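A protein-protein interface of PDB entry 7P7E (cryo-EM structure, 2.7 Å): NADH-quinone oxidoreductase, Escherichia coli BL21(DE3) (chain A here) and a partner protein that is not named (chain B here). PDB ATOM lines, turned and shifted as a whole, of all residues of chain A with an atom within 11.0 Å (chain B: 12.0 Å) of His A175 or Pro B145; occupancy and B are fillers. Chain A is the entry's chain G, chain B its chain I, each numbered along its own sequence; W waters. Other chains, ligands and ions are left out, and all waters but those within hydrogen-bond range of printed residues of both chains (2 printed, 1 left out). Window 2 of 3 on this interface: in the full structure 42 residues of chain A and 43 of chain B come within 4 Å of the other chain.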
ATOM      1  N   ALA A  43       3.540  14.186 -21.879  1.00  0.00           N
ATOM      2  CA  ALA A  43       2.695  14.900 -20.928  1.00  0.00           C
ATOM      3  C   ALA A  43       2.604  16.388 -21.252  1.00  0.00           C
ATOM      4  O   ALA A  43       1.524  16.900 -21.548  1.00  0.00           O
ATOM      5  CB  ALA A  43       3.212  14.690 -19.504  1.00  0.00           C
ATOM      6  N   TRP A  93      -0.002  28.723 -21.059  1.00  0.00           N
ATOM      7  CA  TRP A  93      -0.850  27.937 -20.167  1.00  0.00           C
ATOM      8  C   TRP A  93      -0.108  27.564 -18.893  1.00  0.00           C
ATOM      9  O   TRP A  93      -0.689  27.572 -17.804  1.00  0.00           O
ATOM     10  CB  TRP A  93      -1.344  26.678 -20.876  1.00  0.00           C
ATOM     11  CG  TRP A  93      -2.383  26.926 -21.917  1.00  0.00           C
ATOM     12  CD1 TRP A  93      -3.388  27.841 -21.868  1.00  0.00           C
ATOM     13  CD2 TRP A  93      -2.524  26.241 -23.165  1.00  0.00           C
ATOM     14  NE1 TRP A  93      -4.144  27.773 -23.009  1.00  0.00           N
ATOM     15  CE2 TRP A  93      -3.634  26.798 -23.822  1.00  0.00           C
ATOM     16  CE3 TRP A  93      -1.816  25.211 -23.789  1.00  0.00           C
ATOM     17  CZ2 TRP A  93      -4.053  26.361 -25.075  1.00  0.00           C
ATOM     18  CZ3 TRP A  93      -2.231  24.783 -25.032  1.00  0.00           C
ATOM     19  CH2 TRP A  93      -3.341  25.354 -25.660  1.00  0.00           C
ATOM     20  N   LEU A  94       1.181  27.234 -19.012  1.00  0.00           N
ATOM     21  CA  LEU A  94       1.981  27.012 -17.811  1.00  0.00           C
ATOM     22  C   LEU A  94       2.165  28.296 -17.009  1.00  0.00           C
ATOM     23  O   LEU A  94       2.238  28.249 -15.778  1.00  0.00           O
ATOM     24  CB  LEU A  94       3.337  26.415 -18.182  1.00  0.00           C
ATOM     25  CG  LEU A  94       3.285  25.007 -18.769  1.00  0.00           C
ATOM     26  CD1 LEU A  94       4.681  24.503 -19.056  1.00  0.00           C
ATOM     27  CD2 LEU A  94       2.557  24.071 -17.828  1.00  0.00           C
ATOM     28  N   ASN A  97      -0.746  30.050 -13.998  1.00  0.00           N
ATOM     29  CA  ASN A  97      -0.767  29.800 -12.565  1.00  0.00           C
ATOM     30  C   ASN A  97       0.590  29.968 -11.899  1.00  0.00           C
ATOM     31  O   ASN A  97       0.696  29.750 -10.690  1.00  0.00           O
ATOM     32  CB  ASN A  97      -1.292  28.390 -12.284  1.00  0.00           C
ATOM     33  CG  ASN A  97      -2.733  28.215 -12.696  1.00  0.00           C
ATOM     34  OD1 ASN A  97      -3.592  29.019 -12.347  1.00  0.00           O
ATOM     35  ND2 ASN A  97      -3.007  27.156 -13.445  1.00  0.00           N
ATOM     36  N   ARG A 132      -3.875  29.413  -9.094  1.00  0.00           N
ATOM     37  CA  ARG A 132      -3.981  28.391  -8.066  1.00  0.00           C
ATOM     38  C   ARG A 132      -2.746  28.413  -7.174  1.00  0.00           C
ATOM     39  O   ARG A 132      -1.645  28.763  -7.603  1.00  0.00           O
ATOM     40  CB  ARG A 132      -4.168  27.008  -8.697  1.00  0.00           C
ATOM     41  CG  ARG A 132      -2.994  26.507  -9.530  1.00  0.00           C
ATOM     42  CD  ARG A 132      -2.222  25.424  -8.797  1.00  0.00           C
ATOM     43  NE  ARG A 132      -0.995  25.039  -9.484  1.00  0.00           N
ATOM     44  CZ  ARG A 132       0.163  25.675  -9.373  1.00  0.00           C
ATOM     45  NH1 ARG A 132       0.289  26.759  -8.627  1.00  0.00           N
ATOM     46  NH2 ARG A 132       1.222  25.208 -10.026  1.00  0.00           N
ATOM     47  N   THR A 133      -2.939  28.050  -5.911  1.00  0.00           N
ATOM     48  CA  THR A 133      -1.852  28.012  -4.947  1.00  0.00           C
ATOM     49  C   THR A 133      -1.840  26.669  -4.236  1.00  0.00           C
ATOM     50  O   THR A 133      -2.813  25.912  -4.271  1.00  0.00           O
ATOM     51  CB  THR A 133      -1.952  29.151  -3.922  1.00  0.00           C
ATOM     52  OG1 THR A 133      -3.294  29.249  -3.435  1.00  0.00           O
ATOM     53  CG2 THR A 133      -1.560  30.463  -4.558  1.00  0.00           C
ATOM     54  N   HIS A 134      -0.713  26.378  -3.594  1.00  0.00           N
ATOM     55  CA  HIS A 134      -0.512  25.115  -2.908  1.00  0.00           C
ATOM     56  C   HIS A 134       0.269  25.348  -1.625  1.00  0.00           C
ATOM     57  O   HIS A 134       1.130  26.228  -1.556  1.00  0.00           O
ATOM     58  CB  HIS A 134       0.246  24.114  -3.786  1.00  0.00           C
ATOM     59  CG  HIS A 134      -0.578  23.524  -4.886  1.00  0.00           C
ATOM     60  ND1 HIS A 134      -1.702  22.765  -4.649  1.00  0.00           N
ATOM     61  CD2 HIS A 134      -0.434  23.573  -6.230  1.00  0.00           C
ATOM     62  CE1 HIS A 134      -2.217  22.374  -5.798  1.00  0.00           C
ATOM     63  NE2 HIS A 134      -1.466  22.851  -6.775  1.00  0.00           N
ATOM     64  N   MET A 147       5.609  24.058  -3.977  1.00  0.00           N
ATOM     65  CA  MET A 147       4.663  23.426  -4.889  1.00  0.00           C
ATOM     66  C   MET A 147       3.979  24.419  -5.822  1.00  0.00           C
ATOM     67  O   MET A 147       3.377  23.998  -6.814  1.00  0.00           O
ATOM     68  CB  MET A 147       3.641  22.668  -4.046  1.00  0.00           C
ATOM     69  CG  MET A 147       2.913  21.505  -4.678  1.00  0.00           C
ATOM     70  SD  MET A 147       3.738  20.484  -5.896  1.00  0.00           S
ATOM     71  CE  MET A 147       2.497  20.575  -7.171  1.00  0.00           C
ATOM     72  N   CYS A 150       5.175  24.466  -9.686  1.00  0.00           N
ATOM     73  CA  CYS A 150       5.089  23.255 -10.486  1.00  0.00           C
ATOM     74  C   CYS A 150       4.324  23.488 -11.778  1.00  0.00           C
ATOM     75  O   CYS A 150       3.337  24.226 -11.817  1.00  0.00           O
ATOM     76  CB  CYS A 150       4.429  22.153  -9.675  1.00  0.00           C
ATOM     77  SG  CYS A 150       4.173  20.603 -10.528  1.00  0.00           S
ATOM     78  N   ILE A 151       4.794  22.849 -12.843  1.00  0.00           N
ATOM     79  CA  ILE A 151       4.147  22.886 -14.142  1.00  0.00           C
ATOM     80  C   ILE A 151       3.539  21.538 -14.500  1.00  0.00           C
ATOM     81  O   ILE A 151       3.091  21.350 -15.635  1.00  0.00           O
ATOM     82  CB  ILE A 151       5.122  23.359 -15.230  1.00  0.00           C
ATOM     83  CG1 ILE A 151       6.372  22.481 -15.240  1.00  0.00           C
ATOM     84  CG2 ILE A 151       5.492  24.809 -15.006  1.00  0.00           C
ATOM     85  CD1 ILE A 151       7.173  22.578 -16.496  1.00  0.00           C
ATOM     86  N   ALA A 152       3.515  20.598 -13.546  1.00  0.00           N
ATOM     87  CA  ALA A 152       2.923  19.263 -13.697  1.00  0.00           C
ATOM     88  C   ALA A 152       3.508  18.517 -14.894  1.00  0.00           C
ATOM     89  O   ALA A 152       2.790  18.023 -15.764  1.00  0.00           O
ATOM     90  CB  ALA A 152       1.398  19.335 -13.780  1.00  0.00           C
ATOM     91  N   CYS A 153       4.832  18.452 -14.938  1.00  0.00           N
ATOM     92  CA  CYS A 153       5.524  17.778 -16.023  1.00  0.00           C
ATOM     93  C   CYS A 153       5.840  16.321 -15.715  1.00  0.00           C
ATOM     94  O   CYS A 153       6.342  15.618 -16.597  1.00  0.00           O
ATOM     95  CB  CYS A 153       6.810  18.531 -16.359  1.00  0.00           C
ATOM     96  SG  CYS A 153       8.189  18.190 -15.269  1.00  0.00           S
ATOM     97  N   TYR A 154       5.573  15.867 -14.491  1.00  0.00           N
ATOM     98  CA  TYR A 154       5.680  14.482 -14.036  1.00  0.00           C
ATOM     99  C   TYR A 154       7.102  13.933 -14.076  1.00  0.00           C
ATOM    100  O   TYR A 154       7.284  12.723 -13.954  1.00  0.00           O
ATOM    101  CB  TYR A 154       4.747  13.546 -14.822  1.00  0.00           C
ATOM    102  CG  TYR A 154       3.278  13.819 -14.604  1.00  0.00           C
ATOM    103  CD1 TYR A 154       2.622  14.807 -15.324  1.00  0.00           C
ATOM    104  CD2 TYR A 154       2.547  13.089 -13.680  1.00  0.00           C
ATOM    105  CE1 TYR A 154       1.282  15.063 -15.125  1.00  0.00           C
ATOM    106  CE2 TYR A 154       1.208  13.336 -13.474  1.00  0.00           C
ATOM    107  CZ  TYR A 154       0.582  14.323 -14.200  1.00  0.00           C
ATOM    108  OH  TYR A 154      -0.753  14.575 -14.002  1.00  0.00           O
ATOM    109  N   VAL A 171       2.151  11.489  -7.189  1.00  0.00           N
ATOM    110  CA  VAL A 171       1.253  12.527  -7.673  1.00  0.00           C
ATOM    111  C   VAL A 171      -0.129  12.260  -7.090  1.00  0.00           C
ATOM    112  O   VAL A 171      -0.612  11.122  -7.106  1.00  0.00           O
ATOM    113  CB  VAL A 171       1.233  12.584  -9.213  1.00  0.00           C
ATOM    114  CG1 VAL A 171       1.100  11.193  -9.823  1.00  0.00           C
ATOM    115  CG2 VAL A 171       0.136  13.511  -9.715  1.00  0.00           C
ATOM    116  N   TYR A 172      -0.738  13.300  -6.535  1.00  0.00           N
ATOM    117  CA  TYR A 172      -2.020  13.223  -5.861  1.00  0.00           C
ATOM    118  C   TYR A 172      -2.951  14.262  -6.460  1.00  0.00           C
ATOM    119  O   TYR A 172      -2.528  15.182  -7.162  1.00  0.00           O
ATOM    120  CB  TYR A 172      -1.865  13.447  -4.352  1.00  0.00           C
ATOM    121  CG  TYR A 172      -0.615  12.814  -3.812  1.00  0.00           C
ATOM    122  CD1 TYR A 172      -0.554  11.449  -3.584  1.00  0.00           C
ATOM    123  CD2 TYR A 172       0.517  13.573  -3.568  1.00  0.00           C
ATOM    124  CE1 TYR A 172       0.590  10.862  -3.109  1.00  0.00           C
ATOM    125  CE2 TYR A 172       1.665  12.996  -3.096  1.00  0.00           C
ATOM    126  CZ  TYR A 172       1.697  11.638  -2.868  1.00  0.00           C
ATOM    127  OH  TYR A 172       2.844  11.057  -2.398  1.00  0.00           O
ATOM    128  N   GLY A 173      -4.234  14.099  -6.180  1.00  0.00           N
ATOM    129  CA  GLY A 173      -5.204  15.065  -6.637  1.00  0.00           C
ATOM    130  C   GLY A 173      -5.650  14.808  -8.065  1.00  0.00           C
ATOM    131  O   GLY A 173      -5.575  13.697  -8.585  1.00  0.00           O
ATOM    132  N   ALA A 174      -6.091  15.878  -8.709  1.00  0.00           N
ATOM    133  CA  ALA A 174      -6.857  15.787  -9.937  1.00  0.00           C
ATOM    134  C   ALA A 174      -6.532  17.010 -10.784  1.00  0.00           C
ATOM    135  O   ALA A 174      -5.504  17.663 -10.580  1.00  0.00           O
ATOM    136  CB  ALA A 174      -8.356  15.640  -9.631  1.00  0.00           C
ATOM    137  N   HIS A 175      -7.459  17.359 -11.669  1.00  0.00           N
ATOM    138  CA  HIS A 175      -7.314  18.093 -12.921  1.00  0.00           C
ATOM    139  C   HIS A 175      -6.260  19.191 -12.971  1.00  0.00           C
ATOM    140  O   HIS A 175      -5.214  19.005 -13.591  1.00  0.00           O
ATOM    141  CB  HIS A 175      -8.677  18.724 -13.182  1.00  0.00           C
ATOM    142  CG  HIS A 175      -9.428  19.015 -11.917  1.00  0.00           C
ATOM    143  ND1 HIS A 175      -9.206  20.147 -11.163  1.00  0.00           N
ATOM    144  CD2 HIS A 175     -10.354  18.295 -11.241  1.00  0.00           C
ATOM    145  CE1 HIS A 175      -9.980  20.124 -10.093  1.00  0.00           C
ATOM    146  NE2 HIS A 175     -10.687  19.010 -10.118  1.00  0.00           N
ATOM    147  N   ASP A 176      -6.471  20.298 -12.270  1.00  0.00           N
ATOM    148  CA  ASP A 176      -5.479  21.359 -12.198  1.00  0.00           C
ATOM    149  C   ASP A 176      -4.952  21.510 -10.784  1.00  0.00           C
ATOM    150  O   ASP A 176      -4.174  22.427 -10.508  1.00  0.00           O
ATOM    151  CB  ASP A 176      -6.057  22.680 -12.710  1.00  0.00           C
ATOM    152  CG  ASP A 176      -7.142  23.234 -11.811  1.00  0.00           C
ATOM    153  OD1 ASP A 176      -8.292  22.757 -11.900  1.00  0.00           O
ATOM    154  OD2 ASP A 176      -6.850  24.154 -11.019  1.00  0.00           O
ATOM    155  N   ASN A 177      -5.361  20.618  -9.888  1.00  0.00           N
ATOM    156  CA  ASN A 177      -4.905  20.582  -8.510  1.00  0.00           C
ATOM    157  C   ASN A 177      -3.957  19.411  -8.266  1.00  0.00           C
ATOM    158  O   ASN A 177      -3.921  18.861  -7.164  1.00  0.00           O
ATOM    159  CB  ASN A 177      -6.105  20.507  -7.567  1.00  0.00           C
ATOM    160  CG  ASN A 177      -5.906  21.313  -6.308  1.00  0.00           C
ATOM    161  OD1 ASN A 177      -5.300  22.381  -6.331  1.00  0.00           O
ATOM    162  ND2 ASN A 177      -6.416  20.805  -5.194  1.00  0.00           N
ATOM    163  N   VAL A 178      -3.205  19.004  -9.293  1.00  0.00           N
ATOM    164  CA  VAL A 178      -2.235  17.926  -9.139  1.00  0.00           C
ATOM    165  C   VAL A 178      -1.122  18.369  -8.203  1.00  0.00           C
ATOM    166  O   VAL A 178      -0.575  19.471  -8.332  1.00  0.00           O
ATOM    167  CB  VAL A 178      -1.671  17.487 -10.501  1.00  0.00           C
ATOM    168  CG1 VAL A 178      -2.587  16.483 -11.163  1.00  0.00           C
ATOM    169  CG2 VAL A 178      -1.463  18.684 -11.407  1.00  0.00           C
ATOM    170  N   TYR A 179      -0.791  17.510  -7.247  1.00  0.00           N
ATOM    171  CA  TYR A 179       0.192  17.794  -6.214  1.00  0.00           C
ATOM    172  C   TYR A 179       1.274  16.731  -6.277  1.00  0.00           C
ATOM    173  O   TYR A 179       0.977  15.537  -6.226  1.00  0.00           O
ATOM    174  CB  TYR A 179      -0.471  17.804  -4.836  1.00  0.00           C
ATOM    175  CG  TYR A 179       0.313  18.477  -3.736  1.00  0.00           C
ATOM    176  CD1 TYR A 179       1.361  17.826  -3.103  1.00  0.00           C
ATOM    177  CD2 TYR A 179      -0.025  19.751  -3.305  1.00  0.00           C
ATOM    178  CE1 TYR A 179       2.067  18.433  -2.091  1.00  0.00           C
ATOM    179  CE2 TYR A 179       0.668  20.361  -2.288  1.00  0.00           C
ATOM    180  CZ  TYR A 179       1.718  19.702  -1.688  1.00  0.00           C
ATOM    181  OH  TYR A 179       2.417  20.310  -0.677  1.00  0.00           O
ATOM    182  N   PHE A 180       2.525  17.154  -6.374  1.00  0.00           N
ATOM    183  CA  PHE A 180       3.647  16.230  -6.438  1.00  0.00           C
ATOM    184  C   PHE A 180       4.406  16.309  -5.125  1.00  0.00           C
ATOM    185  O   PHE A 180       4.899  17.378  -4.755  1.00  0.00           O
ATOM    186  CB  PHE A 180       4.553  16.558  -7.625  1.00  0.00           C
ATOM    187  CG  PHE A 180       3.901  16.333  -8.956  1.00  0.00           C
ATOM    188  CD1 PHE A 180       3.114  17.316  -9.532  1.00  0.00           C
ATOM    189  CD2 PHE A 180       4.063  15.135  -9.625  1.00  0.00           C
ATOM    190  CE1 PHE A 180       2.508  17.108 -10.751  1.00  0.00           C
ATOM    191  CE2 PHE A 180       3.461  14.924 -10.846  1.00  0.00           C
ATOM    192  CZ  PHE A 180       2.682  15.911 -11.408  1.00  0.00           C
ATOM    193  N   ALA B 135      -5.654  32.654  -5.717  1.00  0.00           N
ATOM    194  CA  ALA B 135      -6.730  31.936  -5.058  1.00  0.00           C
ATOM    195  C   ALA B 135      -6.196  31.216  -3.827  1.00  0.00           C
ATOM    196  O   ALA B 135      -4.991  31.003  -3.676  1.00  0.00           O
ATOM    197  CB  ALA B 135      -7.380  30.939  -6.016  1.00  0.00           C
ATOM    198  N   LYS B 136      -7.112  30.853  -2.933  1.00  0.00           N
ATOM    199  CA  LYS B 136      -6.737  30.087  -1.758  1.00  0.00           C
ATOM    200  C   LYS B 136      -6.286  28.687  -2.170  1.00  0.00           C
ATOM    201  O   LYS B 136      -6.784  28.133  -3.152  1.00  0.00           O
ATOM    202  CB  LYS B 136      -7.908  29.988  -0.786  1.00  0.00           C
ATOM    203  CG  LYS B 136      -8.336  31.313  -0.191  1.00  0.00           C
ATOM    204  CD  LYS B 136      -7.257  31.888   0.708  1.00  0.00           C
ATOM    205  CE  LYS B 136      -7.775  33.087   1.482  1.00  0.00           C
ATOM    206  NZ  LYS B 136      -9.219  32.951   1.815  1.00  0.00           N
ATOM    207  N   PRO B 137      -5.323  28.108  -1.454  1.00  0.00           N
ATOM    208  CA  PRO B 137      -4.894  26.743  -1.776  1.00  0.00           C
ATOM    209  C   PRO B 137      -5.996  25.733  -1.495  1.00  0.00           C
ATOM    210  O   PRO B 137      -6.681  25.799  -0.473  1.00  0.00           O
ATOM    211  CB  PRO B 137      -3.682  26.520  -0.866  1.00  0.00           C
ATOM    212  CG  PRO B 137      -3.807  27.533   0.206  1.00  0.00           C
ATOM    213  CD  PRO B 137      -4.498  28.710  -0.395  1.00  0.00           C
ATOM    214  N   ILE B 138      -6.163  24.800  -2.424  1.00  0.00           N
ATOM    215  CA  ILE B 138      -7.161  23.744  -2.323  1.00  0.00           C
ATOM    216  C   ILE B 138      -6.425  22.441  -2.058  1.00  0.00           C
ATOM    217  O   ILE B 138      -5.593  22.016  -2.868  1.00  0.00           O
ATOM    218  CB  ILE B 138      -8.016  23.647  -3.595  1.00  0.00           C
ATOM    219  CG1 ILE B 138      -8.763  24.957  -3.835  1.00  0.00           C
ATOM    220  CG2 ILE B 138      -8.989  22.488  -3.493  1.00  0.00           C
ATOM    221  CD1 ILE B 138      -9.366  25.068  -5.207  1.00  0.00           C
ATOM    222  N   ASP B 139      -6.720  21.819  -0.922  1.00  0.00           N
ATOM    223  CA  ASP B 139      -6.119  20.538  -0.592  1.00  0.00           C
ATOM    224  C   ASP B 139      -6.623  19.461  -1.543  1.00  0.00           C
ATOM    225  O   ASP B 139      -7.760  19.502  -2.015  1.00  0.00           O
ATOM    226  CB  ASP B 139      -6.438  20.154   0.853  1.00  0.00           C
ATOM    227  CG  ASP B 139      -5.341  19.327   1.493  1.00  0.00           C
ATOM    228  OD1 ASP B 139      -4.354  19.919   1.978  1.00  0.00           O
ATOM    229  OD2 ASP B 139      -5.461  18.086   1.511  1.00  0.00           O
ATOM    230  N   VAL B 140      -5.752  18.490  -1.831  1.00  0.00           N
ATOM    231  CA  VAL B 140      -6.134  17.389  -2.708  1.00  0.00           C
ATOM    232  C   VAL B 140      -7.113  16.446  -2.029  1.00  0.00           C
ATOM    233  O   VAL B 140      -7.746  15.624  -2.700  1.00  0.00           O
ATOM    234  CB  VAL B 140      -4.888  16.621  -3.187  1.00  0.00           C
ATOM    235  CG1 VAL B 140      -4.060  17.496  -4.099  1.00  0.00           C
ATOM    236  CG2 VAL B 140      -4.063  16.153  -2.000  1.00  0.00           C
ATOM    237  N   LYS B 141      -7.257  16.546  -0.712  1.00  0.00           N
ATOM    238  CA  LYS B 141      -8.194  15.737   0.050  1.00  0.00           C
ATOM    239  C   LYS B 141      -9.584  16.352   0.127  1.00  0.00           C
ATOM    240  O   LYS B 141     -10.447  15.806   0.819  1.00  0.00           O
ATOM    241  CB  LYS B 141      -7.650  15.513   1.462  1.00  0.00           C
ATOM    242  CG  LYS B 141      -6.285  14.852   1.488  1.00  0.00           C
ATOM    243  CD  LYS B 141      -5.988  14.248   2.846  1.00  0.00           C
ATOM    244  CE  LYS B 141      -5.161  15.191   3.699  1.00  0.00           C
ATOM    245  NZ  LYS B 141      -6.009  16.193   4.397  1.00  0.00           N
ATOM    246  N   SER B 142      -9.817  17.468  -0.562  1.00  0.00           N
ATOM    247  CA  SER B 142     -11.105  18.145  -0.504  1.00  0.00           C
ATOM    248  C   SER B 142     -12.191  17.319  -1.183  1.00  0.00           C
ATOM    249  O   SER B 142     -11.944  16.594  -2.149  1.00  0.00           O
ATOM    250  CB  SER B 142     -11.014  19.521  -1.160  1.00  0.00           C
ATOM    251  OG  SER B 142     -11.134  19.424  -2.567  1.00  0.00           O
ATOM    252  N   LEU B 143     -13.411  17.438  -0.658  1.00  0.00           N
ATOM    253  CA  LEU B 143     -14.534  16.649  -1.146  1.00  0.00           C
ATOM    254  C   LEU B 143     -15.088  17.156  -2.469  1.00  0.00           C
ATOM    255  O   LEU B 143     -15.770  16.399  -3.167  1.00  0.00           O
ATOM    256  CB  LEU B 143     -15.649  16.631  -0.102  1.00  0.00           C
ATOM    257  CG  LEU B 143     -15.219  16.295   1.323  1.00  0.00           C
ATOM    258  CD1 LEU B 143     -16.335  16.616   2.298  1.00  0.00           C
ATOM    259  CD2 LEU B 143     -14.812  14.837   1.427  1.00  0.00           C
ATOM    260  N   LEU B 144     -14.824  18.408  -2.822  1.00  0.00           N
ATOM    261  CA  LEU B 144     -15.333  18.944  -4.074  1.00  0.00           C
ATOM    262  C   LEU B 144     -14.565  18.347  -5.251  1.00  0.00           C
ATOM    263  O   LEU B 144     -13.347  18.163  -5.170  1.00  0.00           O
ATOM    264  CB  LEU B 144     -15.218  20.466  -4.092  1.00  0.00           C
ATOM    265  CG  LEU B 144     -16.197  21.212  -3.187  1.00  0.00           C
ATOM    266  CD1 LEU B 144     -15.896  22.699  -3.183  1.00  0.00           C
ATOM    267  CD2 LEU B 144     -17.626  20.951  -3.626  1.00  0.00           C
ATOM    268  N   PRO B 145     -15.249  18.028  -6.360  1.00  0.00           N
ATOM    269  CA  PRO B 145     -14.592  17.466  -7.546  1.00  0.00           C
ATOM    270  C   PRO B 145     -13.701  18.483  -8.255  1.00  0.00           C
ATOM    271  O   PRO B 145     -13.951  19.683  -8.138  1.00  0.00           O
ATOM    272  CB  PRO B 145     -15.767  17.055  -8.444  1.00  0.00           C
ATOM    273  CG  PRO B 145     -16.975  17.073  -7.563  1.00  0.00           C
ATOM    274  CD  PRO B 145     -16.707  18.113  -6.532  1.00  0.00           C
HETATM  275  O   HOH W   1      -5.724  27.350  -5.342  1.00  0.00           O
HETATM  276  O   HOH W   2      -4.852  24.487  -5.156  1.00  0.00           O
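The side-chain hydroxyl (OG1) of Thr A133 sits close to the backbone nitrogen (N) of Pro B137. O of Ala B135 lies within hydrogen-bond range of OG1 of Thr A133 (2.5 Å). O of Ile B138 lies within hydrogen-bond range of ND2 of Asn A177 (2.7 Å).
Water W2 lies within hydrogen-bond range of the side-chain amide oxygen of Asn A177 (2.5 Å), the backbone carbonyl oxygen of Thr A133 (2.6 Å) and the backbone NH of Ile B138 (3.0 Å). Water W1 lies within hydrogen-bond range of O of Lys B136 and N of Thr A133.
Of the 23 printed residues of chain A, 5 touch a printed residue of chain B. Printed residues of chain A that touch a printed residue of chain B: Thr A133, Gly A173, His A175, Asn A177 and Tyr A179. Of the 11 printed residues of chain B, 7 touch a printed residue of chain A. Hydrophobic or aromatic side chains of chain B that line the printed part of chain A: Pro B137, Ile B138 and Val B140. Among the printed residues, 10 pairs touch across the chains. Among the printed residues, no Asp or Glu carboxylate lies within 4 Å of a Lys or Arg side-chain nitrogen of the other chain.
The side-chain carboxylate (OD1) of Asp A176 sits at hydrogen-bond distance from a ring nitrogen (ND1) of His A175, 2.9 Å away. The side-chain carboxylate of Asp B139 is in salt-bridge range of the side-chain amino group of Lys B141. The backbone carbonyl oxygen of Tyr A179 sits at hydrogen-bond distance from the backbone NH of Tyr A172 (2.8 Å). The backbone carbonyl oxygen (O) of Asp B139 sits close to the side-chain hydroxyl (OG) of Ser B142.
Asn A97 touches none of the printed residues of chain B. Of chain B, only Val B140 comes within 4 Å of Gly A173. Of chain B, only Pro B145 comes within 4 Å of His A175. No residue of chain B comes within 4 Å of Asp A176. Asn A177 touches three residues of chain B. No residue of chain B comes within 4 Å of Val A178. Printed residues of chain B within 4 Å of Tyr A179: Val B140 (3.7 Å). Printed residues of chain A within 4 Å of Pro B137: Thr A133. No residue of chain A comes within 4 Å of Leu B144. Of chain A, only His A175 (3.6 Å) comes within 4 Å of Pro B145. The nearest residue of chain B that does not touch His A175 is Leu B144 (5.7 Å). The nearest printed residue of chain B that does not touch Thr A133 is Asp B139 (6.6 Å).
Among the printed residues, pairs that only touch across the chains: Thr A133 with Lys B136 (3.3 Å), Asn A177 with Val B140 (3.4 Å), His A175 with Pro B145 (3.6 Å), Tyr A179 with Val B140 (3.7 Å), Asn A177 with Asp B139 (3.7 Å), Gly A173 with Val B140 (3.7 Å) and Thr A133 with Ile B138 (3.98 Å).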
